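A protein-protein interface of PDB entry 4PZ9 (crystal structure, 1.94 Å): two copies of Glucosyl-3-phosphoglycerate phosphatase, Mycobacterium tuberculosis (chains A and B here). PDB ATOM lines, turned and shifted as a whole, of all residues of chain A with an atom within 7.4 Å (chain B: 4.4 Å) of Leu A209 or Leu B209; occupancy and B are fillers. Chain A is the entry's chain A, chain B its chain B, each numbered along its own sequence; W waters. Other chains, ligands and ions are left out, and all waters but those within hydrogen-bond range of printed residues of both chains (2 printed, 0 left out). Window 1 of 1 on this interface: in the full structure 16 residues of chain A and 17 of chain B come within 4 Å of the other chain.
Among the printed residues, pairs that only touch across the chains: Trp A212 with Val B211 (3.3 Å), Val A211 with Trp B212 (3.3 Å), Asp A210 with Trp B212 (3.4 Å), Arg A208 with Ala B180 (3.5 Å), Ala A180 with Arg B208 (3.6 Å), Leu A209 with Trp B212 (3.6 Å), Leu A209 with Leu B209 (3.7 Å), Ala A180 with Leu B171 (3.8 Å), Gly A183 with Asp B210 (3.8 Å), Leu A171 with Ala B180 (3.9 Å), Asn A213 with Val B211 (3.9 Å) and Leu A209 with Leu B181 (3.9 Å).
The backbone carbonyl oxygen (O) of Gly B182 sits close to the indole nitrogen (NE1) of Trp B212, 3.1 Å away.
O of Gly A183 lies within hydrogen-bond range of NE1 of Trp A212 (3.4 Å).
The side-chain hydroxyl (OG1) of Thr A190 sits at hydrogen-bond distance from the backbone NH (N) of Asn A213, at 3.1 Å.
NE2 of Gln A191 sits at hydrogen-bond distance from OD2 of Asp A210, at 2.9 Å.
The backbone NH of Gln B191 sits at hydrogen-bond distance from the backbone carbonyl oxygen of Val B211 (2.8 Å).
The backbone carbonyl oxygen of Gln B191 lies within hydrogen-bond range of the backbone NH of Asp B210 (2.8 Å).
Water W1 lies within hydrogen-bond range of OD1 of Asp B210 (2.5 Å) and N of Gly A183 (2.9 Å).
Water W2 lies within hydrogen-bond range of the backbone carbonyl oxygen of Gly A183 (2.9 Å), the side-chain amide nitrogen of Asn A213 (3.3 Å) and the backbone carbonyl oxygen of Asp B210 (3.4 Å).
Leu A209 touches just these residues of chain B: Ala B180 (2.6 Å), Leu B181 (3.9 Å), Gly B182 (2.8 Å), Leu B209 (3.7 Å) and Trp B212 (3.6 Å).
Printed residues of chain A within 4 Å of Leu B209: Ala A180 (2.8 Å), Gly A182 (2.9 Å), Leu A209 (3.7 Å) and Trp A212 (3.4 Å).
Printed residues of chain A within 4 Å of Asp B210: Gly A183 (3.8 Å), Trp A212 (3.2 Å) and Asn A213 (2.9 Å).
Printed residues of chain A within 4 Å of Leu B171: Ala A180.
Printed residues of chain B within 4 Å of Arg A208: Ala B180 (3.5 Å).
Gln B191 touches none of the printed residues of chain A.
The nearest printed residue of chain B that does not touch Leu A209 is Val B211 (6.9 Å).
The nearest residue of chain A that does not touch Leu B209 is Leu A181 (4.1 Å).
The nearest printed residue of chain B that does not touch Arg A110 is Leu B209 (6.9 Å).
Of the 12 printed residues of chain B, 9 touch a printed residue of chain A.
Printed residues of chain B that touch a printed residue of chain A: Leu B171, Ala B180, Leu B181, Gly B182, Arg B208, Leu B209, Asp B210, Val B211 and Trp B212.
Hydrophobic or aromatic side chains of chain B that line the printed part of chain A: Leu B171, Ala B180, Leu B209, Val B211 and Trp B212.
Along chain B the printed residues that touch a printed residue of chain A span positions 171 to 212.
Printed residues of chain A that touch a printed residue of chain B: Arg A110, Leu A171, Ala A180, Gly A182, Gly A183, Arg A208, Leu A209, Asp A210, Val A211, Trp A212 and Asn A213.
Among the printed residues, 21 pairs touch across the chains.
Ala A180 touches Arg B208, and with the chains exchanged Arg A208 touches Ala B180.
Ala A180 touches Leu B209, and with the chains exchanged Leu A209 touches Ala B180.
Leu A209 touches its own counterpart, Leu B209.
Leu A209 touches Trp B212, and with the chains exchanged Trp A212 touches Leu B209.
Positions printed for both chains: 171, 180, 181, 182, 190, 191, 192, 208, 209, 210, 211 and 212.
Of the 21 pairs that touch across the chains among the printed residues, 16 have their exchanged pair printed and touching as well.
ND2 of Asn A213 lies within hydrogen-bond range of O of Asp B210 (2.9 Å).
The backbone carbonyl oxygen of Ala A180 sits at hydrogen-bond distance from the backbone NH of Leu B209.
The backbone carbonyl oxygen of Asp B210 lies close to the indole nitrogen of Trp A212, at 3.5 Å.
The backbone carbonyl oxygen (O) of Leu A209 lies within hydrogen-bond range of the backbone NH (N) of Gly B182 (2.8 Å).
The guanidinium group of Arg A110 sits close to the guanidinium group of Arg B208, 3.1 Å away.
The indole nitrogen (NE1) of Trp A212 lies within hydrogen-bond range of the backbone carbonyl oxygen (O) of Leu B209, 3.4 Å away.
The backbone NH of Leu A209 lies within hydrogen-bond range of the backbone carbonyl oxygen of Ala B180 (2.6 Å).
The backbone carbonyl oxygen of Trp A212 lies within hydrogen-bond range of the backbone NH of Trp B212 (2.9 Å).
N of Gly A182 is in hydrogen-bond range of O of Leu B209, at 2.9 Å.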
ATOM      1  N   ARG A 110      20.692  11.281  20.247  1.00  0.00           N
ATOM      2  CA  ARG A 110      21.316  10.186  20.986  1.00  0.00           C
ATOM      3  C   ARG A 110      21.081  10.325  22.488  1.00  0.00           C
ATOM      4  O   ARG A 110      21.082   9.333  23.221  1.00  0.00           O
ATOM      5  CB  ARG A 110      22.823  10.101  20.690  1.00  0.00           C
ATOM      6  CG  ARG A 110      23.429   8.747  21.075  1.00  0.00           C
ATOM      7  CD  ARG A 110      24.877   8.846  21.567  1.00  0.00           C
ATOM      8  NE  ARG A 110      24.960   9.171  22.989  1.00  0.00           N
ATOM      9  CZ  ARG A 110      24.915   8.279  23.979  1.00  0.00           C
ATOM     10  NH1 ARG A 110      24.773   6.979  23.732  1.00  0.00           N
ATOM     11  NH2 ARG A 110      25.006   8.689  25.232  1.00  0.00           N
ATOM     12  N   ILE A 163      19.248  -3.470  20.582  1.00  0.00           N
ATOM     13  CA  ILE A 163      19.867  -4.049  21.775  1.00  0.00           C
ATOM     14  C   ILE A 163      19.807  -3.035  22.916  1.00  0.00           C
ATOM     15  O   ILE A 163      19.471  -3.381  24.060  1.00  0.00           O
ATOM     16  CB  ILE A 163      21.379  -4.441  21.547  1.00  0.00           C
ATOM     17  CG1 ILE A 163      21.564  -5.390  20.369  1.00  0.00           C
ATOM     18  CG2 ILE A 163      21.988  -5.051  22.797  1.00  0.00           C
ATOM     19  CD1 ILE A 163      20.523  -6.427  20.286  1.00  0.00           C
ATOM     20  N   SER A 167      17.399  -3.591  26.018  1.00  0.00           N
ATOM     21  CA  SER A 167      18.126  -3.890  27.252  1.00  0.00           C
ATOM     22  C   SER A 167      17.728  -2.876  28.321  1.00  0.00           C
ATOM     23  O   SER A 167      17.471  -3.246  29.459  1.00  0.00           O
ATOM     24  CB  SER A 167      19.648  -3.922  27.048  1.00  0.00           C
ATOM     25  OG  SER A 167      20.041  -4.984  26.172  1.00  0.00           O
ATOM     26  N   LEU A 171      15.870  -3.894  31.815  1.00  0.00           N
ATOM     27  CA  LEU A 171      16.528  -3.525  33.073  1.00  0.00           C
ATOM     28  C   LEU A 171      15.665  -2.539  33.859  1.00  0.00           C
ATOM     29  O   LEU A 171      15.949  -2.262  35.022  1.00  0.00           O
ATOM     30  CB  LEU A 171      17.885  -2.879  32.786  1.00  0.00           C
ATOM     31  CG  LEU A 171      18.951  -3.746  32.134  1.00  0.00           C
ATOM     32  CD1 LEU A 171      20.044  -2.852  31.578  1.00  0.00           C
ATOM     33  CD2 LEU A 171      19.525  -4.733  33.143  1.00  0.00           C
ATOM     34  N   PRO A 179      20.303   6.590  27.484  1.00  0.00           N
ATOM     35  CA  PRO A 179      21.527   6.895  26.734  1.00  0.00           C
ATOM     36  C   PRO A 179      22.825   6.479  27.427  1.00  0.00           C
ATOM     37  O   PRO A 179      23.898   6.615  26.839  1.00  0.00           O
ATOM     38  CB  PRO A 179      21.499   8.426  26.620  1.00  0.00           C
ATOM     39  CG  PRO A 179      20.048   8.778  26.668  1.00  0.00           C
ATOM     40  CD  PRO A 179      19.455   7.793  27.639  1.00  0.00           C
ATOM     41  N   ALA A 180      22.747   5.996  28.655  1.00  0.00           N
ATOM     42  CA  ALA A 180      23.955   5.507  29.316  1.00  0.00           C
ATOM     43  C   ALA A 180      24.497   4.228  28.654  1.00  0.00           C
ATOM     44  O   ALA A 180      25.660   3.855  28.862  1.00  0.00           O
ATOM     45  CB  ALA A 180      23.694   5.292  30.794  1.00  0.00           C
ATOM     46  N   LEU A 181      23.658   3.557  27.863  1.00  0.00           N
ATOM     47  CA  LEU A 181      24.076   2.357  27.141  1.00  0.00           C
ATOM     48  C   LEU A 181      24.680   2.762  25.796  1.00  0.00           C
ATOM     49  O   LEU A 181      24.033   3.437  24.997  1.00  0.00           O
ATOM     50  CB  LEU A 181      22.893   1.395  26.953  1.00  0.00           C
ATOM     51  CG  LEU A 181      22.323   0.837  28.265  1.00  0.00           C
ATOM     52  CD1 LEU A 181      21.153  -0.077  28.011  1.00  0.00           C
ATOM     53  CD2 LEU A 181      23.380   0.078  29.055  1.00  0.00           C
ATOM     54  N   GLY A 182      25.932   2.375  25.565  1.00  0.00           N
ATOM     55  CA  GLY A 182      26.658   2.822  24.391  1.00  0.00           C
ATOM     56  C   GLY A 182      26.390   2.006  23.141  1.00  0.00           C
ATOM     57  O   GLY A 182      25.299   1.442  22.957  1.00  0.00           O
ATOM     58  N   GLY A 183      27.390   1.964  22.266  1.00  0.00           N
ATOM     59  CA  GLY A 183      27.259   1.297  20.985  1.00  0.00           C
ATOM     60  C   GLY A 183      27.640  -0.166  21.070  1.00  0.00           C
ATOM     61  O   GLY A 183      28.262  -0.606  22.042  1.00  0.00           O
ATOM     62  N   MET A 184      27.215  -0.933  20.071  1.00  0.00           N
ATOM     63  CA  MET A 184      27.598  -2.332  19.947  1.00  0.00           C
ATOM     64  C   MET A 184      28.440  -2.430  18.687  1.00  0.00           C
ATOM     65  O   MET A 184      28.088  -1.830  17.672  1.00  0.00           O
ATOM     66  CB  MET A 184      26.355  -3.202  19.749  1.00  0.00           C
ATOM     67  CG  MET A 184      25.361  -3.176  20.877  1.00  0.00           C
ATOM     68  SD  MET A 184      25.879  -4.289  22.169  1.00  0.00           S
ATOM     69  CE  MET A 184      25.329  -5.840  21.450  1.00  0.00           C
ATOM     70  N   THR A 190      25.565  -9.100  23.590  1.00  0.00           N
ATOM     71  CA  THR A 190      25.222  -8.615  24.910  1.00  0.00           C
ATOM     72  C   THR A 190      24.403  -9.710  25.559  1.00  0.00           C
ATOM     73  O   THR A 190      23.692 -10.437  24.869  1.00  0.00           O
ATOM     74  CB  THR A 190      24.427  -7.315  24.766  1.00  0.00           C
ATOM     75  OG1 THR A 190      25.356  -6.233  24.654  1.00  0.00           O
ATOM     76  CG2 THR A 190      23.511  -7.080  25.958  1.00  0.00           C
ATOM     77  N   GLN A 191      24.540  -9.880  26.870  1.00  0.00           N
ATOM     78  CA  GLN A 191      23.757 -10.885  27.572  1.00  0.00           C
ATOM     79  C   GLN A 191      23.100 -10.297  28.817  1.00  0.00           C
ATOM     80  O   GLN A 191      23.732  -9.547  29.570  1.00  0.00           O
ATOM     81  CB  GLN A 191      24.654 -12.064  27.969  1.00  0.00           C
ATOM     82  CG  GLN A 191      24.008 -13.070  28.927  1.00  0.00           C
ATOM     83  CD  GLN A 191      24.958 -14.214  29.269  1.00  0.00           C
ATOM     84  OE1 GLN A 191      25.519 -14.844  28.377  1.00  0.00           O
ATOM     85  NE2 GLN A 191      25.144 -14.476  30.563  1.00  0.00           N
ATOM     86  N   LEU A 192      21.825 -10.630  29.012  1.00  0.00           N
ATOM     87  CA  LEU A 192      21.086 -10.241  30.216  1.00  0.00           C
ATOM     88  C   LEU A 192      20.633 -11.516  30.890  1.00  0.00           C
ATOM     89  O   LEU A 192      20.490 -12.550  30.232  1.00  0.00           O
ATOM     90  CB  LEU A 192      19.840  -9.425  29.843  1.00  0.00           C
ATOM     91  CG  LEU A 192      19.866  -7.900  29.747  1.00  0.00           C
ATOM     92  CD1 LEU A 192      21.069  -7.385  29.014  1.00  0.00           C
ATOM     93  CD2 LEU A 192      18.578  -7.380  29.092  1.00  0.00           C
ATOM     94  N   SER A 193      20.408 -11.444  32.199  1.00  0.00           N
ATOM     95  CA  SER A 193      19.831 -12.550  32.938  1.00  0.00           C
ATOM     96  C   SER A 193      18.601 -12.072  33.670  1.00  0.00           C
ATOM     97  O   SER A 193      18.641 -11.060  34.386  1.00  0.00           O
ATOM     98  CB  SER A 193      20.824 -13.097  33.953  1.00  0.00           C
ATOM     99  OG  SER A 193      21.880 -13.758  33.297  1.00  0.00           O
ATOM    100  N   TRP A 207      15.769  -8.273  35.578  1.00  0.00           N
ATOM    101  CA  TRP A 207      16.875  -8.456  34.645  1.00  0.00           C
ATOM    102  C   TRP A 207      18.126  -7.717  35.079  1.00  0.00           C
ATOM    103  O   TRP A 207      18.045  -6.615  35.616  1.00  0.00           O
ATOM    104  CB  TRP A 207      16.445  -7.966  33.263  1.00  0.00           C
ATOM    105  CG  TRP A 207      15.269  -8.752  32.760  1.00  0.00           C
ATOM    106  CD1 TRP A 207      13.944  -8.534  33.036  1.00  0.00           C
ATOM    107  CD2 TRP A 207      15.318  -9.905  31.911  1.00  0.00           C
ATOM    108  NE1 TRP A 207      13.169  -9.473  32.390  1.00  0.00           N
ATOM    109  CE2 TRP A 207      13.990 -10.324  31.693  1.00  0.00           C
ATOM    110  CE3 TRP A 207      16.359 -10.610  31.306  1.00  0.00           C
ATOM    111  CZ2 TRP A 207      13.677 -11.445  30.911  1.00  0.00           C
ATOM    112  CZ3 TRP A 207      16.048 -11.715  30.512  1.00  0.00           C
ATOM    113  CH2 TRP A 207      14.724 -12.118  30.319  1.00  0.00           C
ATOM    114  N   ARG A 208      19.283  -8.334  34.839  1.00  0.00           N
ATOM    115  CA  ARG A 208      20.560  -7.666  35.031  1.00  0.00           C
ATOM    116  C   ARG A 208      21.444  -7.830  33.800  1.00  0.00           C
ATOM    117  O   ARG A 208      21.282  -8.769  33.011  1.00  0.00           O
ATOM    118  CB  ARG A 208      21.270  -8.162  36.299  1.00  0.00           C
ATOM    119  CG  ARG A 208      21.932  -9.542  36.184  1.00  0.00           C
ATOM    120  CD  ARG A 208      22.547  -9.966  37.519  1.00  0.00           C
ATOM    121  NE  ARG A 208      21.528 -10.327  38.509  1.00  0.00           N
ATOM    122  CZ  ARG A 208      21.749 -11.109  39.563  1.00  0.00           C
ATOM    123  NH1 ARG A 208      22.964 -11.606  39.772  1.00  0.00           N
ATOM    124  NH2 ARG A 208      20.762 -11.397  40.406  1.00  0.00           N
ATOM    125  N   LEU A 209      22.358  -6.887  33.629  1.00  0.00           N
ATOM    126  CA  LEU A 209      23.302  -6.894  32.521  1.00  0.00           C
ATOM    127  C   LEU A 209      24.543  -7.727  32.872  1.00  0.00           C
ATOM    128  O   LEU A 209      25.351  -7.325  33.721  1.00  0.00           O
ATOM    129  CB  LEU A 209      23.702  -5.446  32.185  1.00  0.00           C
ATOM    130  CG  LEU A 209      24.790  -5.298  31.115  1.00  0.00           C
ATOM    131  CD1 LEU A 209      24.277  -5.797  29.757  1.00  0.00           C
ATOM    132  CD2 LEU A 209      25.247  -3.872  31.009  1.00  0.00           C
ATOM    133  N   ASP A 210      24.681  -8.896  32.244  1.00  0.00           N
ATOM    134  CA  ASP A 210      25.830  -9.768  32.499  1.00  0.00           C
ATOM    135  C   ASP A 210      27.022  -9.336  31.656  1.00  0.00           C
ATOM    136  O   ASP A 210      28.165  -9.338  32.131  1.00  0.00           O
ATOM    137  CB  ASP A 210      25.519 -11.225  32.110  1.00  0.00           C
ATOM    138  CG  ASP A 210      24.373 -11.828  32.903  1.00  0.00           C
ATOM    139  OD1 ASP A 210      24.114 -11.389  34.043  1.00  0.00           O
ATOM    140  OD2 ASP A 210      23.733 -12.768  32.371  1.00  0.00           O
ATOM    141  N   VAL A 211      26.750  -9.019  30.389  1.00  0.00           N
ATOM    142  CA  VAL A 211      27.786  -8.650  29.418  1.00  0.00           C
ATOM    143  C   VAL A 211      27.234  -7.607  28.445  1.00  0.00           C
ATOM    144  O   VAL A 211      26.138  -7.785  27.930  1.00  0.00           O
ATOM    145  CB  VAL A 211      28.255  -9.872  28.582  1.00  0.00           C
ATOM    146  CG1 VAL A 211      29.250  -9.427  27.498  1.00  0.00           C
ATOM    147  CG2 VAL A 211      28.903 -10.926  29.464  1.00  0.00           C
ATOM    148  N   TRP A 212      27.980  -6.525  28.202  1.00  0.00           N
ATOM    149  CA  TRP A 212      27.611  -5.541  27.187  1.00  0.00           C
ATOM    150  C   TRP A 212      28.722  -5.427  26.123  1.00  0.00           C
ATOM    151  O   TRP A 212      29.870  -5.078  26.448  1.00  0.00           O
ATOM    152  CB  TRP A 212      27.294  -4.152  27.812  1.00  0.00           C
ATOM    153  CG  TRP A 212      26.982  -3.115  26.744  1.00  0.00           C
ATOM    154  CD1 TRP A 212      27.867  -2.246  26.153  1.00  0.00           C
ATOM    155  CD2 TRP A 212      25.717  -2.879  26.116  1.00  0.00           C
ATOM    156  NE1 TRP A 212      27.221  -1.491  25.204  1.00  0.00           N
ATOM    157  CE2 TRP A 212      25.898  -1.861  25.164  1.00  0.00           C
ATOM    158  CE3 TRP A 212      24.442  -3.442  26.266  1.00  0.00           C
ATOM    159  CZ2 TRP A 212      24.852  -1.387  24.349  1.00  0.00           C
ATOM    160  CZ3 TRP A 212      23.400  -2.959  25.465  1.00  0.00           C
ATOM    161  CH2 TRP A 212      23.614  -1.945  24.525  1.00  0.00           C
ATOM    162  N   ASN A 213      28.391  -5.754  24.869  1.00  0.00           N
ATOM    163  CA  ASN A 213      29.290  -5.502  23.737  1.00  0.00           C
ATOM    164  C   ASN A 213      30.609  -6.281  23.796  1.00  0.00           C
ATOM    165  O   ASN A 213      31.707  -5.711  23.723  1.00  0.00           O
ATOM    166  CB  ASN A 213      29.524  -3.986  23.583  1.00  0.00           C
ATOM    167  CG  ASN A 213      30.298  -3.633  22.326  1.00  0.00           C
ATOM    168  OD1 ASN A 213      30.144  -4.283  21.291  1.00  0.00           O
ATOM    169  ND2 ASN A 213      31.138  -2.595  22.411  1.00  0.00           N
ATOM    170  N   LEU B 171      28.175   6.822  35.127  1.00  0.00           N
ATOM    171  CA  LEU B 171      27.021   6.831  34.208  1.00  0.00           C
ATOM    172  C   LEU B 171      25.836   7.650  34.742  1.00  0.00           C
ATOM    173  O   LEU B 171      24.906   7.978  34.000  1.00  0.00           O
ATOM    174  CB  LEU B 171      26.558   5.404  33.941  1.00  0.00           C
ATOM    175  CG  LEU B 171      27.539   4.463  33.234  1.00  0.00           C
ATOM    176  CD1 LEU B 171      26.955   3.058  33.216  1.00  0.00           C
ATOM    177  CD2 LEU B 171      27.859   4.921  31.817  1.00  0.00           C
ATOM    178  N   ALA B 180      21.470  -3.187  38.186  1.00  0.00           N
ATOM    179  CA  ALA B 180      21.374  -3.585  36.790  1.00  0.00           C
ATOM    180  C   ALA B 180      22.711  -4.111  36.262  1.00  0.00           C
ATOM    181  O   ALA B 180      22.737  -4.899  35.309  1.00  0.00           O
ATOM    182  CB  ALA B 180      20.862  -2.429  35.937  1.00  0.00           C
ATOM    183  N   LEU B 181      23.814  -3.702  36.896  1.00  0.00           N
ATOM    184  CA  LEU B 181      25.146  -4.157  36.495  1.00  0.00           C
ATOM    185  C   LEU B 181      25.536  -5.480  37.154  1.00  0.00           C
ATOM    186  O   LEU B 181      25.741  -5.546  38.370  1.00  0.00           O
ATOM    187  CB  LEU B 181      26.192  -3.078  36.789  1.00  0.00           C
ATOM    188  CG  LEU B 181      25.871  -1.739  36.115  1.00  0.00           C
ATOM    189  CD1 LEU B 181      26.932  -0.697  36.410  1.00  0.00           C
ATOM    190  CD2 LEU B 181      25.716  -1.921  34.612  1.00  0.00           C
ATOM    191  N   GLY B 182      25.648  -6.532  36.343  1.00  0.00           N
ATOM    192  CA  GLY B 182      25.932  -7.865  36.846  1.00  0.00           C
ATOM    193  C   GLY B 182      27.396  -7.978  37.220  1.00  0.00           C
ATOM    194  O   GLY B 182      28.213  -7.195  36.734  1.00  0.00           O
ATOM    195  N   THR B 190      35.899  -3.686  31.536  1.00  0.00           N
ATOM    196  CA  THR B 190      34.761  -2.835  31.232  1.00  0.00           C
ATOM    197  C   THR B 190      35.298  -1.523  30.689  1.00  0.00           C
ATOM    198  O   THR B 190      36.377  -1.084  31.088  1.00  0.00           O
ATOM    199  CB  THR B 190      33.931  -2.625  32.504  1.00  0.00           C
ATOM    200  OG1 THR B 190      33.063  -3.746  32.679  1.00  0.00           O
ATOM    201  CG2 THR B 190      33.104  -1.341  32.438  1.00  0.00           C
ATOM    202  N   GLN B 191      34.595  -0.921  29.733  1.00  0.00           N
ATOM    203  CA  GLN B 191      35.039   0.360  29.209  1.00  0.00           C
ATOM    204  C   GLN B 191      33.925   1.406  29.232  1.00  0.00           C
ATOM    205  O   GLN B 191      32.800   1.153  28.778  1.00  0.00           O
ATOM    206  CB  GLN B 191      35.604   0.199  27.783  1.00  0.00           C
ATOM    207  CG  GLN B 191      36.187   1.502  27.225  1.00  0.00           C
ATOM    208  CD  GLN B 191      36.750   1.331  25.836  1.00  0.00           C
ATOM    209  OE1 GLN B 191      37.738   0.630  25.640  1.00  0.00           O
ATOM    210  NE2 GLN B 191      36.114   1.960  24.858  1.00  0.00           N
ATOM    211  N   LEU B 192      34.231   2.578  29.785  1.00  0.00           N
ATOM    212  CA  LEU B 192      33.304   3.711  29.769  1.00  0.00           C
ATOM    213  C   LEU B 192      33.924   4.790  28.895  1.00  0.00           C
ATOM    214  O   LEU B 192      35.145   4.908  28.837  1.00  0.00           O
ATOM    215  CB  LEU B 192      33.096   4.274  31.185  1.00  0.00           C
ATOM    216  CG  LEU B 192      31.993   3.765  32.120  1.00  0.00           C
ATOM    217  CD1 LEU B 192      31.804   2.285  31.982  1.00  0.00           C
ATOM    218  CD2 LEU B 192      32.272   4.138  33.585  1.00  0.00           C
ATOM    219  N   ARG B 208      29.229   7.123  28.900  1.00  0.00           N
ATOM    220  CA  ARG B 208      28.405   6.052  28.348  1.00  0.00           C
ATOM    221  C   ARG B 208      29.144   4.742  28.500  1.00  0.00           C
ATOM    222  O   ARG B 208      30.373   4.718  28.555  1.00  0.00           O
ATOM    223  CB  ARG B 208      28.025   6.324  26.882  1.00  0.00           C
ATOM    224  CG  ARG B 208      29.175   6.230  25.876  1.00  0.00           C
ATOM    225  CD  ARG B 208      28.693   6.522  24.440  1.00  0.00           C
ATOM    226  NE  ARG B 208      28.353   7.935  24.263  1.00  0.00           N
ATOM    227  CZ  ARG B 208      28.286   8.571  23.092  1.00  0.00           C
ATOM    228  NH1 ARG B 208      28.548   7.928  21.957  1.00  0.00           N
ATOM    229  NH2 ARG B 208      27.978   9.866  23.055  1.00  0.00           N
ATOM    230  N   LEU B 209      28.394   3.646  28.581  1.00  0.00           N
ATOM    231  CA  LEU B 209      28.987   2.331  28.751  1.00  0.00           C
ATOM    232  C   LEU B 209      29.318   1.705  27.400  1.00  0.00           C
ATOM    233  O   LEU B 209      28.401   1.369  26.628  1.00  0.00           O
ATOM    234  CB  LEU B 209      28.011   1.421  29.507  1.00  0.00           C
ATOM    235  CG  LEU B 209      28.414  -0.045  29.650  1.00  0.00           C
ATOM    236  CD1 LEU B 209      29.598  -0.167  30.589  1.00  0.00           C
ATOM    237  CD2 LEU B 209      27.241  -0.879  30.162  1.00  0.00           C
ATOM    238  N   ASP B 210      30.608   1.522  27.121  1.00  0.00           N
ATOM    239  CA  ASP B 210      31.045   0.964  25.836  1.00  0.00           C
ATOM    240  C   ASP B 210      31.099  -0.560  25.886  1.00  0.00           C
ATOM    241  O   ASP B 210      30.679  -1.236  24.956  1.00  0.00           O
ATOM    242  CB  ASP B 210      32.439   1.483  25.437  1.00  0.00           C
ATOM    243  CG  ASP B 210      32.490   2.981  25.247  1.00  0.00           C
ATOM    244  OD1 ASP B 210      31.453   3.617  24.923  1.00  0.00           O
ATOM    245  OD2 ASP B 210      33.603   3.535  25.422  1.00  0.00           O
ATOM    246  N   VAL B 211      31.637  -1.091  26.984  1.00  0.00           N
ATOM    247  CA  VAL B 211      31.863  -2.529  27.146  1.00  0.00           C
ATOM    248  C   VAL B 211      31.615  -2.872  28.601  1.00  0.00           C
ATOM    249  O   VAL B 211      32.129  -2.186  29.477  1.00  0.00           O
ATOM    250  CB  VAL B 211      33.331  -2.890  26.828  1.00  0.00           C
ATOM    251  CG1 VAL B 211      33.626  -4.336  27.196  1.00  0.00           C
ATOM    252  CG2 VAL B 211      33.652  -2.620  25.350  1.00  0.00           C
ATOM    253  N   TRP B 212      30.806  -3.895  28.875  1.00  0.00           N
ATOM    254  CA  TRP B 212      30.673  -4.383  30.242  1.00  0.00           C
ATOM    255  C   TRP B 212      31.065  -5.860  30.344  1.00  0.00           C
ATOM    256  O   TRP B 212      30.469  -6.706  29.673  1.00  0.00           O
ATOM    257  CB  TRP B 212      29.248  -4.179  30.792  1.00  0.00           C
ATOM    258  CG  TRP B 212      29.126  -4.742  32.185  1.00  0.00           C
ATOM    259  CD1 TRP B 212      28.628  -5.956  32.543  1.00  0.00           C
ATOM    260  CD2 TRP B 212      29.549  -4.106  33.405  1.00  0.00           C
ATOM    261  NE1 TRP B 212      28.717  -6.119  33.911  1.00  0.00           N
ATOM    262  CE2 TRP B 212      29.273  -4.993  34.460  1.00  0.00           C
ATOM    263  CE3 TRP B 212      30.145  -2.876  33.693  1.00  0.00           C
ATOM    264  CZ2 TRP B 212      29.571  -4.686  35.803  1.00  0.00           C
ATOM    265  CZ3 TRP B 212      30.433  -2.563  35.028  1.00  0.00           C
ATOM    266  CH2 TRP B 212      30.147  -3.465  36.060  1.00  0.00           C
HETATM  267  O   HOH W   1      30.032   2.992  22.920  1.00  0.00           O
HETATM  268  O   HOH W   2      30.844   0.695  22.135  1.00  0.00           O
